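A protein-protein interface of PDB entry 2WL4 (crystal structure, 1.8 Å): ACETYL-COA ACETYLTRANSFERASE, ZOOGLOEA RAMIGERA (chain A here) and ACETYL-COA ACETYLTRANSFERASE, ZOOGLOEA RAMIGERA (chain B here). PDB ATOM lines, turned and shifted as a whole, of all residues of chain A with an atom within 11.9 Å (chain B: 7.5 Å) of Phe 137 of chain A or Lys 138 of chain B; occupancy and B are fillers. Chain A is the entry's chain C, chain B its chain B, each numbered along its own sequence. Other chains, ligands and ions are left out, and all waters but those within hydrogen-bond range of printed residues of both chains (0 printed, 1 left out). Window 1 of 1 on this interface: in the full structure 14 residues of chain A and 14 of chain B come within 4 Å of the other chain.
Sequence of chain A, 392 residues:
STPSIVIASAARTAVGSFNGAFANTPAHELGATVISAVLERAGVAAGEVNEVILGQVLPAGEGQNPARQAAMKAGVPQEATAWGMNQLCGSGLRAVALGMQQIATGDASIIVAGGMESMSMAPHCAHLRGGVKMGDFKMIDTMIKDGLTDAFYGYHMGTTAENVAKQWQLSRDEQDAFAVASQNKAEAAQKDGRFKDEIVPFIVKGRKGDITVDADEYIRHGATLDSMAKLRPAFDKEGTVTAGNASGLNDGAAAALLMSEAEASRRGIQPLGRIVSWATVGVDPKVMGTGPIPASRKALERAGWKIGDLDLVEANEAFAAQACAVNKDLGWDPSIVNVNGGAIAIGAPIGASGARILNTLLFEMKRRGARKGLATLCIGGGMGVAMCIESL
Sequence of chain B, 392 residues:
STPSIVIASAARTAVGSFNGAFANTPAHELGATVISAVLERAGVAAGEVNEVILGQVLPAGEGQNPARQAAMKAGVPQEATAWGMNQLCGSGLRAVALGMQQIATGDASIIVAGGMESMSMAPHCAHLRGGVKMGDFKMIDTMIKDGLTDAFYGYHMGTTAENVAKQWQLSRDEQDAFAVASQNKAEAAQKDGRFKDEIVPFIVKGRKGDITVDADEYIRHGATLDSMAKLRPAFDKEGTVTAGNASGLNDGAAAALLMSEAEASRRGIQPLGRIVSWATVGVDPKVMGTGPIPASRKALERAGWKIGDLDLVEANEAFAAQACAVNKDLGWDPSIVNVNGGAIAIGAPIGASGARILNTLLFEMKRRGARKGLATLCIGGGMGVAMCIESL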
ATOM      1  N   HIS A 124     -10.118  22.118 -22.687  1.00  0.00           N
ATOM      2  CA  HIS A 124      -9.210  21.013 -22.927  1.00  0.00           C
ATOM      3  C   HIS A 124      -9.959  19.737 -22.591  1.00  0.00           C
ATOM      4  O   HIS A 124     -10.816  19.733 -21.705  1.00  0.00           O
ATOM      5  CB  HIS A 124      -7.976  21.132 -22.037  1.00  0.00           C
ATOM      6  CG  HIS A 124      -7.066  22.258 -22.414  1.00  0.00           C
ATOM      7  ND1 HIS A 124      -7.439  23.582 -22.306  1.00  0.00           N
ATOM      8  CD2 HIS A 124      -5.797  22.266 -22.884  1.00  0.00           C
ATOM      9  CE1 HIS A 124      -6.440  24.351 -22.697  1.00  0.00           C
ATOM     10  NE2 HIS A 124      -5.429  23.576 -23.054  1.00  0.00           N
ATOM     11  N   CYS A 125      -9.623  18.651 -23.281  1.00  0.00           N
ATOM     12  CA  CYS A 125     -10.325  17.388 -23.086  1.00  0.00           C
ATOM     13  C   CYS A 125      -9.399  16.170 -23.006  1.00  0.00           C
ATOM     14  O   CYS A 125      -8.233  16.249 -23.386  1.00  0.00           O
ATOM     15  CB  CYS A 125     -11.306  17.182 -24.234  1.00  0.00           C
ATOM     16  SG  CYS A 125     -10.522  17.152 -25.861  1.00  0.00           S
ATOM     17  N   ALA A 126      -9.938  15.045 -22.530  1.00  0.00           N
ATOM     18  CA  ALA A 126      -9.232  13.775 -22.579  1.00  0.00           C
ATOM     19  C   ALA A 126     -10.236  12.627 -22.529  1.00  0.00           C
ATOM     20  O   ALA A 126     -11.159  12.646 -21.717  1.00  0.00           O
ATOM     21  CB  ALA A 126      -8.208  13.648 -21.407  1.00  0.00           C
ATOM     22  N   HIS A 127     -10.061  11.626 -23.386  1.00  0.00           N
ATOM     23  CA  HIS A 127     -10.945  10.470 -23.352  1.00  0.00           C
ATOM     24  C   HIS A 127     -10.643   9.622 -22.127  1.00  0.00           C
ATOM     25  O   HIS A 127      -9.555   9.046 -22.002  1.00  0.00           O
ATOM     26  CB  HIS A 127     -10.816   9.629 -24.613  1.00  0.00           C
ATOM     27  CG  HIS A 127     -11.706   8.426 -24.613  1.00  0.00           C
ATOM     28  ND1 HIS A 127     -11.281   7.181 -25.027  1.00  0.00           N
ATOM     29  CD2 HIS A 127     -12.994   8.273 -24.222  1.00  0.00           C
ATOM     30  CE1 HIS A 127     -12.274   6.319 -24.911  1.00  0.00           C
ATOM     31  NE2 HIS A 127     -13.325   6.955 -24.422  1.00  0.00           N
ATOM     32  N   LEU A 128     -11.608   9.523 -21.226  1.00  0.00           N
ATOM     33  CA  LEU A 128     -11.315   8.996 -19.890  1.00  0.00           C
ATOM     34  C   LEU A 128     -12.167   7.829 -19.452  1.00  0.00           C
ATOM     35  O   LEU A 128     -12.102   7.410 -18.293  1.00  0.00           O
ATOM     36  CB  LEU A 128     -11.466  10.116 -18.868  1.00  0.00           C
ATOM     37  CG  LEU A 128     -10.489  11.271 -19.007  1.00  0.00           C
ATOM     38  CD1 LEU A 128     -10.907  12.391 -18.072  1.00  0.00           C
ATOM     39  CD2 LEU A 128      -9.092  10.770 -18.686  1.00  0.00           C
ATOM     40  N   ARG A 129     -12.961   7.300 -20.372  1.00  0.00           N
ATOM     41  CA  ARG A 129     -13.814   6.155 -20.075  1.00  0.00           C
ATOM     42  C   ARG A 129     -13.038   4.883 -19.707  1.00  0.00           C
ATOM     43  O   ARG A 129     -13.578   3.988 -19.055  1.00  0.00           O
ATOM     44  CB  ARG A 129     -14.784   5.903 -21.233  1.00  0.00           C
ATOM     45  CG  ARG A 129     -16.110   6.616 -21.035  1.00  0.00           C
ATOM     46  CD  ARG A 129     -16.914   6.734 -22.313  1.00  0.00           C
ATOM     47  NE  ARG A 129     -16.950   8.114 -22.791  1.00  0.00           N
ATOM     48  CZ  ARG A 129     -17.564   9.105 -22.157  1.00  0.00           C
ATOM     49  NH1 ARG A 129     -18.202   8.877 -21.011  1.00  0.00           N
ATOM     50  NH2 ARG A 129     -17.556  10.326 -22.674  1.00  0.00           N
ATOM     51  N   GLY A 130     -11.769   4.808 -20.095  1.00  0.00           N
ATOM     52  CA  GLY A 130     -10.971   3.625 -19.812  1.00  0.00           C
ATOM     53  C   GLY A 130     -10.559   3.513 -18.356  1.00  0.00           C
ATOM     54  O   GLY A 130     -10.579   2.422 -17.780  1.00  0.00           O
ATOM     55  N   GLY A 131     -10.199   4.644 -17.754  1.00  0.00           N
ATOM     56  CA  GLY A 131      -9.730   4.656 -16.380  1.00  0.00           C
ATOM     57  C   GLY A 131      -8.247   4.349 -16.328  1.00  0.00           C
ATOM     58  O   GLY A 131      -7.847   3.236 -15.994  1.00  0.00           O
ATOM     59  N   VAL A 132      -7.436   5.346 -16.661  1.00  0.00           N
ATOM     60  CA  VAL A 132      -5.989   5.179 -16.784  1.00  0.00           C
ATOM     61  C   VAL A 132      -5.369   4.427 -15.604  1.00  0.00           C
ATOM     62  O   VAL A 132      -5.357   4.923 -14.475  1.00  0.00           O
ATOM     63  CB  VAL A 132      -5.297   6.546 -16.960  1.00  0.00           C
ATOM     64  CG1 VAL A 132      -3.868   6.371 -17.470  1.00  0.00           C
ATOM     65  CG2 VAL A 132      -6.101   7.409 -17.914  1.00  0.00           C
ATOM     66  N   LYS A 133      -4.845   3.236 -15.884  1.00  0.00           N
ATOM     67  CA  LYS A 133      -4.303   2.344 -14.862  1.00  0.00           C
ATOM     68  C   LYS A 133      -3.010   2.865 -14.229  1.00  0.00           C
ATOM     69  O   LYS A 133      -2.804   2.734 -13.019  1.00  0.00           O
ATOM     70  CB  LYS A 133      -4.062   0.960 -15.452  1.00  0.00           C
ATOM     71  CG  LYS A 133      -3.125   0.120 -14.627  1.00  0.00           C
ATOM     72  CD  LYS A 133      -2.329  -0.841 -15.491  1.00  0.00           C
ATOM     73  CE  LYS A 133      -1.033  -1.204 -14.804  1.00  0.00           C
ATOM     74  NZ  LYS A 133      -1.259  -2.177 -13.696  1.00  0.00           N
ATOM     75  N   MET A 134      -2.128   3.410 -15.062  1.00  0.00           N
ATOM     76  CA  MET A 134      -0.965   4.180 -14.596  1.00  0.00           C
ATOM     77  C   MET A 134      -0.303   4.948 -15.735  1.00  0.00           C
ATOM     78  O   MET A 134      -0.437   4.588 -16.911  1.00  0.00           O
ATOM     79  CB  MET A 134       0.069   3.304 -13.888  1.00  0.00           C
ATOM     80  CG  MET A 134       0.980   2.501 -14.808  1.00  0.00           C
ATOM     81  SD  MET A 134       2.231   1.571 -13.866  1.00  0.00           S
ATOM     82  CE  MET A 134       3.073   0.712 -15.193  1.00  0.00           C
ATOM     83  N   GLY A 135       0.419   6.003 -15.374  1.00  0.00           N
ATOM     84  CA  GLY A 135       1.080   6.858 -16.346  1.00  0.00           C
ATOM     85  C   GLY A 135       0.279   8.117 -16.636  1.00  0.00           C
ATOM     86  O   GLY A 135      -0.930   8.147 -16.423  1.00  0.00           O
ATOM     87  N   ASP A 136       0.966   9.154 -17.092  1.00  0.00           N
ATOM     88  CA  ASP A 136       0.337  10.444 -17.340  1.00  0.00           C
ATOM     89  C   ASP A 136      -0.542  10.273 -18.567  1.00  0.00           C
ATOM     90  O   ASP A 136      -0.320   9.371 -19.371  1.00  0.00           O
ATOM     91  CB  ASP A 136       1.367  11.523 -17.640  1.00  0.00           C
ATOM     92  CG  ASP A 136       2.489  11.569 -16.643  1.00  0.00           C
ATOM     93  OD1 ASP A 136       2.285  11.189 -15.472  1.00  0.00           O
ATOM     94  OD2 ASP A 136       3.589  11.992 -17.047  1.00  0.00           O
ATOM     95  N   PHE A 137      -1.555  11.113 -18.697  1.00  0.00           N
ATOM     96  CA  PHE A 137      -2.293  11.197 -19.953  1.00  0.00           C
ATOM     97  C   PHE A 137      -2.472  12.662 -20.325  1.00  0.00           C
ATOM     98  O   PHE A 137      -2.440  13.543 -19.467  1.00  0.00           O
ATOM     99  CB  PHE A 137      -3.623  10.433 -19.901  1.00  0.00           C
ATOM    100  CG  PHE A 137      -4.596  10.952 -18.882  1.00  0.00           C
ATOM    101  CD1 PHE A 137      -4.576  10.479 -17.579  1.00  0.00           C
ATOM    102  CD2 PHE A 137      -5.544  11.904 -19.231  1.00  0.00           C
ATOM    103  CE1 PHE A 137      -5.479  10.957 -16.636  1.00  0.00           C
ATOM    104  CE2 PHE A 137      -6.446  12.384 -18.300  1.00  0.00           C
ATOM    105  CZ  PHE A 137      -6.417  11.911 -17.003  1.00  0.00           C
ATOM    106  N   LYS A 138      -2.613  12.932 -21.616  1.00  0.00           N
ATOM    107  CA  LYS A 138      -2.645  14.316 -22.072  1.00  0.00           C
ATOM    108  C   LYS A 138      -4.015  14.968 -21.922  1.00  0.00           C
ATOM    109  O   LYS A 138      -5.051  14.330 -22.114  1.00  0.00           O
ATOM    110  CB  LYS A 138      -2.142  14.438 -23.515  1.00  0.00           C
ATOM    111  CG  LYS A 138      -0.635  14.283 -23.654  1.00  0.00           C
ATOM    112  CD  LYS A 138      -0.143  14.735 -25.022  1.00  0.00           C
ATOM    113  CE  LYS A 138       1.342  14.445 -25.196  1.00  0.00           C
ATOM    114  NZ  LYS A 138       1.814  14.695 -26.589  1.00  0.00           N
ATOM    115  N   MET A 139      -3.997  16.240 -21.540  1.00  0.00           N
ATOM    116  CA  MET A 139      -5.172  17.092 -21.635  1.00  0.00           C
ATOM    117  C   MET A 139      -5.025  17.932 -22.894  1.00  0.00           C
ATOM    118  O   MET A 139      -4.179  18.831 -22.959  1.00  0.00           O
ATOM    119  CB  MET A 139      -5.311  17.970 -20.387  1.00  0.00           C
ATOM    120  CG  MET A 139      -5.850  17.194 -19.188  1.00  0.00           C
ATOM    121  SD  MET A 139      -7.562  16.736 -19.474  1.00  0.00           S
ATOM    122  CE  MET A 139      -7.898  15.738 -18.027  1.00  0.00           C
ATOM    123  N   ILE A 140      -5.839  17.626 -23.901  1.00  0.00           N
ATOM    124  CA  ILE A 140      -5.700  18.237 -25.222  1.00  0.00           C
ATOM    125  C   ILE A 140      -6.472  19.541 -25.373  1.00  0.00           C
ATOM    126  O   ILE A 140      -7.673  19.618 -25.079  1.00  0.00           O
ATOM    127  CB  ILE A 140      -6.178  17.285 -26.336  1.00  0.00           C
ATOM    128  CG1 ILE A 140      -5.383  15.976 -26.313  1.00  0.00           C
ATOM    129  CG2 ILE A 140      -6.086  17.958 -27.693  1.00  0.00           C
ATOM    130  CD1 ILE A 140      -3.944  16.131 -26.729  1.00  0.00           C
ATOM    131  N   ASP A 141      -5.774  20.560 -25.863  1.00  0.00           N
ATOM    132  CA  ASP A 141      -6.388  21.845 -26.145  1.00  0.00           C
ATOM    133  C   ASP A 141      -7.248  21.715 -27.390  1.00  0.00           C
ATOM    134  O   ASP A 141      -6.736  21.721 -28.510  1.00  0.00           O
ATOM    135  CB  ASP A 141      -5.304  22.899 -26.361  1.00  0.00           C
ATOM    136  CG  ASP A 141      -5.845  24.299 -26.328  1.00  0.00           C
ATOM    137  OD1 ASP A 141      -6.936  24.534 -26.905  1.00  0.00           O
ATOM    138  OD2 ASP A 141      -5.176  25.169 -25.726  1.00  0.00           O
ATOM    139  N   HIS B 124      -4.197  11.148 -10.215  1.00  0.00           N
ATOM    140  CA  HIS B 124      -3.530  11.933 -11.235  1.00  0.00           C
ATOM    141  C   HIS B 124      -3.784  13.399 -10.881  1.00  0.00           C
ATOM    142  O   HIS B 124      -4.800  13.723 -10.269  1.00  0.00           O
ATOM    143  CB  HIS B 124      -4.131  11.621 -12.608  1.00  0.00           C
ATOM    144  CG  HIS B 124      -3.710  10.295 -13.166  1.00  0.00           C
ATOM    145  ND1 HIS B 124      -4.095   9.095 -12.610  1.00  0.00           N
ATOM    146  CD2 HIS B 124      -2.917   9.988 -14.223  1.00  0.00           C
ATOM    147  CE1 HIS B 124      -3.581   8.101 -13.317  1.00  0.00           C
ATOM    148  NE2 HIS B 124      -2.854   8.612 -14.291  1.00  0.00           N
ATOM    149  N   CYS B 125      -2.893  14.287 -11.292  1.00  0.00           N
ATOM    150  CA  CYS B 125      -3.035  15.683 -10.896  1.00  0.00           C
ATOM    151  C   CYS B 125      -2.530  16.655 -11.938  1.00  0.00           C
ATOM    152  O   CYS B 125      -1.865  16.271 -12.904  1.00  0.00           O
ATOM    153  CB  CYS B 125      -2.301  15.942  -9.572  1.00  0.00           C
ATOM    154  SG  CYS B 125      -0.483  15.953  -9.735  1.00  0.00           S
ATOM    155  N   ALA B 126      -2.863  17.927 -11.738  1.00  0.00           N
ATOM    156  CA  ALA B 126      -2.400  18.984 -12.624  1.00  0.00           C
ATOM    157  C   ALA B 126      -2.519  20.320 -11.922  1.00  0.00           C
ATOM    158  O   ALA B 126      -3.504  20.572 -11.251  1.00  0.00           O
ATOM    159  CB  ALA B 126      -3.212  18.993 -13.927  1.00  0.00           C
ATOM    160  N   HIS B 127      -1.508  21.163 -12.088  1.00  0.00           N
ATOM    161  CA  HIS B 127      -1.560  22.528 -11.571  1.00  0.00           C
ATOM    162  C   HIS B 127      -2.315  23.403 -12.552  1.00  0.00           C
ATOM    163  O   HIS B 127      -1.832  23.659 -13.648  1.00  0.00           O
ATOM    164  CB  HIS B 127      -0.152  23.088 -11.362  1.00  0.00           C
ATOM    165  CG  HIS B 127      -0.133  24.522 -10.936  1.00  0.00           C
ATOM    166  ND1 HIS B 127       0.549  25.509 -11.636  1.00  0.00           N
ATOM    167  CD2 HIS B 127      -0.752  25.165  -9.918  1.00  0.00           C
ATOM    168  CE1 HIS B 127       0.386  26.666 -11.037  1.00  0.00           C
ATOM    169  NE2 HIS B 127      -0.412  26.491  -9.988  1.00  0.00           N
ATOM    170  N   LEU B 128      -3.485  23.877 -12.130  1.00  0.00           N
ATOM    171  CA  LEU B 128      -4.430  24.539 -13.017  1.00  0.00           C
ATOM    172  C   LEU B 128      -4.825  25.944 -12.556  1.00  0.00           C
ATOM    173  O   LEU B 128      -5.781  26.518 -13.088  1.00  0.00           O
ATOM    174  CB  LEU B 128      -5.687  23.681 -13.136  1.00  0.00           C
ATOM    175  CG  LEU B 128      -5.472  22.262 -13.687  1.00  0.00           C
ATOM    176  CD1 LEU B 128      -6.759  21.480 -13.661  1.00  0.00           C
ATOM    177  CD2 LEU B 128      -4.931  22.344 -15.107  1.00  0.00           C
ATOM    178  N   VAL B 132      -4.202  27.362 -18.205  1.00  0.00           N
ATOM    179  CA  VAL B 132      -3.348  27.025 -19.339  1.00  0.00           C
ATOM    180  C   VAL B 132      -3.811  27.785 -20.580  1.00  0.00           C
ATOM    181  O   VAL B 132      -4.798  27.421 -21.218  1.00  0.00           O
ATOM    182  CB  VAL B 132      -3.311  25.504 -19.594  1.00  0.00           C
ATOM    183  CG1 VAL B 132      -2.696  25.201 -20.949  1.00  0.00           C
ATOM    184  CG2 VAL B 132      -2.530  24.808 -18.482  1.00  0.00           C
ATOM    185  N   GLY B 135      -2.432  25.200 -25.655  1.00  0.00           N
ATOM    186  CA  GLY B 135      -1.555  24.051 -25.832  1.00  0.00           C
ATOM    187  C   GLY B 135      -1.866  22.924 -24.860  1.00  0.00           C
ATOM    188  O   GLY B 135      -2.482  23.143 -23.821  1.00  0.00           O
ATOM    189  N   ASP B 136      -1.438  21.711 -25.190  1.00  0.00           N
ATOM    190  CA  ASP B 136      -1.734  20.557 -24.342  1.00  0.00           C
ATOM    191  C   ASP B 136      -0.993  20.610 -23.011  1.00  0.00           C
ATOM    192  O   ASP B 136       0.001  21.330 -22.864  1.00  0.00           O
ATOM    193  CB  ASP B 136      -1.408  19.246 -25.072  1.00  0.00           C
ATOM    194  CG  ASP B 136      -2.204  19.080 -26.354  1.00  0.00           C
ATOM    195  OD1 ASP B 136      -3.199  19.808 -26.532  1.00  0.00           O
ATOM    196  OD2 ASP B 136      -1.835  18.223 -27.186  1.00  0.00           O
ATOM    197  N   PHE B 137      -1.493  19.846 -22.044  1.00  0.00           N
ATOM    198  CA  PHE B 137      -0.830  19.676 -20.758  1.00  0.00           C
ATOM    199  C   PHE B 137      -1.197  18.309 -20.188  1.00  0.00           C
ATOM    200  O   PHE B 137      -2.269  17.782 -20.464  1.00  0.00           O
ATOM    201  CB  PHE B 137      -1.236  20.781 -19.781  1.00  0.00           C
ATOM    202  CG  PHE B 137      -2.584  20.567 -19.143  1.00  0.00           C
ATOM    203  CD1 PHE B 137      -3.705  21.190 -19.646  1.00  0.00           C
ATOM    204  CD2 PHE B 137      -2.723  19.751 -18.027  1.00  0.00           C
ATOM    205  CE1 PHE B 137      -4.946  21.004 -19.059  1.00  0.00           C
ATOM    206  CE2 PHE B 137      -3.966  19.556 -17.440  1.00  0.00           C
ATOM    207  CZ  PHE B 137      -5.073  20.181 -17.953  1.00  0.00           C
ATOM    208  N   LYS B 138      -0.315  17.749 -19.375  1.00  0.00           N
ATOM    209  CA  LYS B 138      -0.525  16.402 -18.850  1.00  0.00           C
ATOM    210  C   LYS B 138      -1.370  16.383 -17.570  1.00  0.00           C
ATOM    211  O   LYS B 138      -1.287  17.289 -16.753  1.00  0.00           O
ATOM    212  CB  LYS B 138       0.831  15.758 -18.557  1.00  0.00           C
ATOM    213  CG  LYS B 138       2.017  16.543 -19.105  1.00  0.00           C
ATOM    214  CD  LYS B 138       3.336  15.825 -18.879  1.00  0.00           C
ATOM    215  CE  LYS B 138       3.634  14.822 -19.986  1.00  0.00           C
ATOM    216  NZ  LYS B 138       4.060  15.480 -21.256  1.00  0.00           N
ATOM    217  N   MET B 139      -2.193  15.353 -17.409  1.00  0.00           N
ATOM    218  CA  MET B 139      -2.591  14.943 -16.073  1.00  0.00           C
ATOM    219  C   MET B 139      -1.519  13.963 -15.599  1.00  0.00           C
ATOM    220  O   MET B 139      -1.270  12.939 -16.244  1.00  0.00           O
ATOM    221  CB  MET B 139      -3.970  14.292 -16.078  1.00  0.00           C
ATOM    222  CG  MET B 139      -5.090  15.277 -16.216  1.00  0.00           C
ATOM    223  SD  MET B 139      -5.434  16.139 -14.672  1.00  0.00           S
ATOM    224  CE  MET B 139      -6.201  14.817 -13.737  1.00  0.00           C
ATOM    225  N   ILE B 140      -0.874  14.302 -14.494  1.00  0.00           N
ATOM    226  CA  ILE B 140       0.289  13.573 -14.016  1.00  0.00           C
ATOM    227  C   ILE B 140      -0.077  12.464 -13.027  1.00  0.00           C
ATOM    228  O   ILE B 140      -0.774  12.703 -12.069  1.00  0.00           O
ATOM    229  CB  ILE B 140       1.286  14.550 -13.356  1.00  0.00           C
ATOM    230  CG1 ILE B 140       1.719  15.608 -14.384  1.00  0.00           C
ATOM    231  CG2 ILE B 140       2.501  13.814 -12.836  1.00  0.00           C
ATOM    232  CD1 ILE B 140       2.539  15.040 -15.516  1.00  0.00           C
ATOM    233  N   ASP B 141       0.427  11.255 -13.251  1.00  0.00           N
ATOM    234  CA  ASP B 141       0.225  10.186 -12.285  1.00  0.00           C
ATOM    235  C   ASP B 141       1.125  10.445 -11.063  1.00  0.00           C
ATOM    236  O   ASP B 141       2.330  10.288 -11.146  1.00  0.00           O
ATOM    237  CB  ASP B 141       0.546   8.831 -12.951  1.00  0.00           C
ATOM    238  CG  ASP B 141       0.101   7.654 -12.128  1.00  0.00           C
ATOM    239  OD1 ASP B 141       0.070   7.773 -10.884  1.00  0.00           O
ATOM    240  OD2 ASP B 141      -0.195   6.594 -12.721  1.00  0.00           O
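O of Gly 135 of chain A is in hydrogen-bond range of NE2 of His 124 of chain B (2.9 Å).
OD1 of Asp 136 of chain B is in hydrogen-bond range of N of Asp 141 of chain A (2.8 Å).
OD1 of Asp 136 of chain A is in hydrogen-bond range of N of Asp 141 of chain B (2.9 Å).
The backbone NH of Gly 135 of chain A lies within hydrogen-bond range of the side-chain carboxylate of Asp 141 of chain B, at 2.8 Å.
N of Met 139 of chain B sits at hydrogen-bond distance from O of Phe 137 of chain A (2.8 Å).
O of Gly 135 of chain B sits at hydrogen-bond distance from NE2 of His 124 of chain A (3.1 Å).
The backbone NH (N) of Gly 135 of chain B is in hydrogen-bond range of the side-chain carboxylate (OD2) of Asp 141 of chain A, 2.7 Å away.
The backbone NH of Met 139 of chain A lies within hydrogen-bond range of the backbone carbonyl oxygen of Phe 137 of chain B (2.6 Å).
O of Cys 125 of chain A lies within hydrogen-bond range of N of Ile 140 of chain A, 2.8 Å away.
A ring nitrogen (NE2) of His 124 of chain A lies within hydrogen-bond range of the side-chain carboxylate of Asp 141 of chain A (3.1 Å).
O of Cys 125 of chain B is in hydrogen-bond range of N of Ile 140 of chain B, at 2.7 Å.
Among the printed residues, pairs that only touch across the chains: Ile 140 of chain A with Asp 136 of chain B (3.0 Å), Met 134 of chain A with Asp 141 of chain B (3.2 Å), Asp 136 of chain A with Met 139 of chain B (3.2 Å), Met 139 of chain A with Asp 136 of chain B (3.3 Å), Met 139 of chain A with Met 139 of chain B (3.4 Å), Asp 136 of chain A with Ile 140 of chain B (3.4 Å), Phe 137 of chain A with Lys 138 of chain B (3.5 Å), Lys 138 of chain A with Phe 137 of chain B (3.6 Å), Phe 137 of chain A with His 124 of chain B (3.7 Å), His 124 of chain A with Val 132 of chain B (3.8 Å) and Val 132 of chain A with His 124 of chain B (3.8 Å).
Phe 137 of chain A touches just these residues of chain B: His 124 (3.7 Å), Lys 138 (3.5 Å) and Met 139 (2.8 Å).
Of chain A, only Phe 137 comes within 4 Å of Lys 138 of chain B.
Of chain A, only Val 132, Gly 135 and Phe 137 come within 4 Å of His 124 of chain B.
No residue of chain A comes within 4 Å of Cys 125 of chain B.
Ala 126 of chain B touches none of the printed residues of chain A.
Met 139 of chain B touches just these residues of chain A: Asp 136, Phe 137 and Met 139.
Of chain A, only Asp 136 comes within 4 Å of Ile 140 of chain B.
Of the printed residues of chain B, Met 139 of chain A touches Asp 136, Phe 137 and Met 139.
Of the printed residues of chain B, Lys 138 of chain A touches Phe 137 (3.6 Å).
Of the printed residues of chain B, Gly 135 of chain A touches His 124 (2.9 Å) and Asp 141 (2.8 Å).
His 127 of chain B touches none of the printed residues of chain A.
The nearest residue of chain B that does not touch Phe 137 of chain A is Phe 137 of chain B (4.4 Å).
The nearest residue of chain A that does not touch Lys 138 of chain B is Asp 136 of chain A (4.1 Å).
The nearest printed residue of chain A that does not touch Asp 136 of chain B is Lys 138 of chain A (4.4 Å).
Of the 18 printed residues of chain A, 10 touch a printed residue of chain B.
Along chain A the printed residues that touch a printed residue of chain B span positions 124 to 141.
Hydrophobic or aromatic side chains of chain B that line the printed part of chain A: His 124, Val 132, Phe 137, Met 139 and Ile 140.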
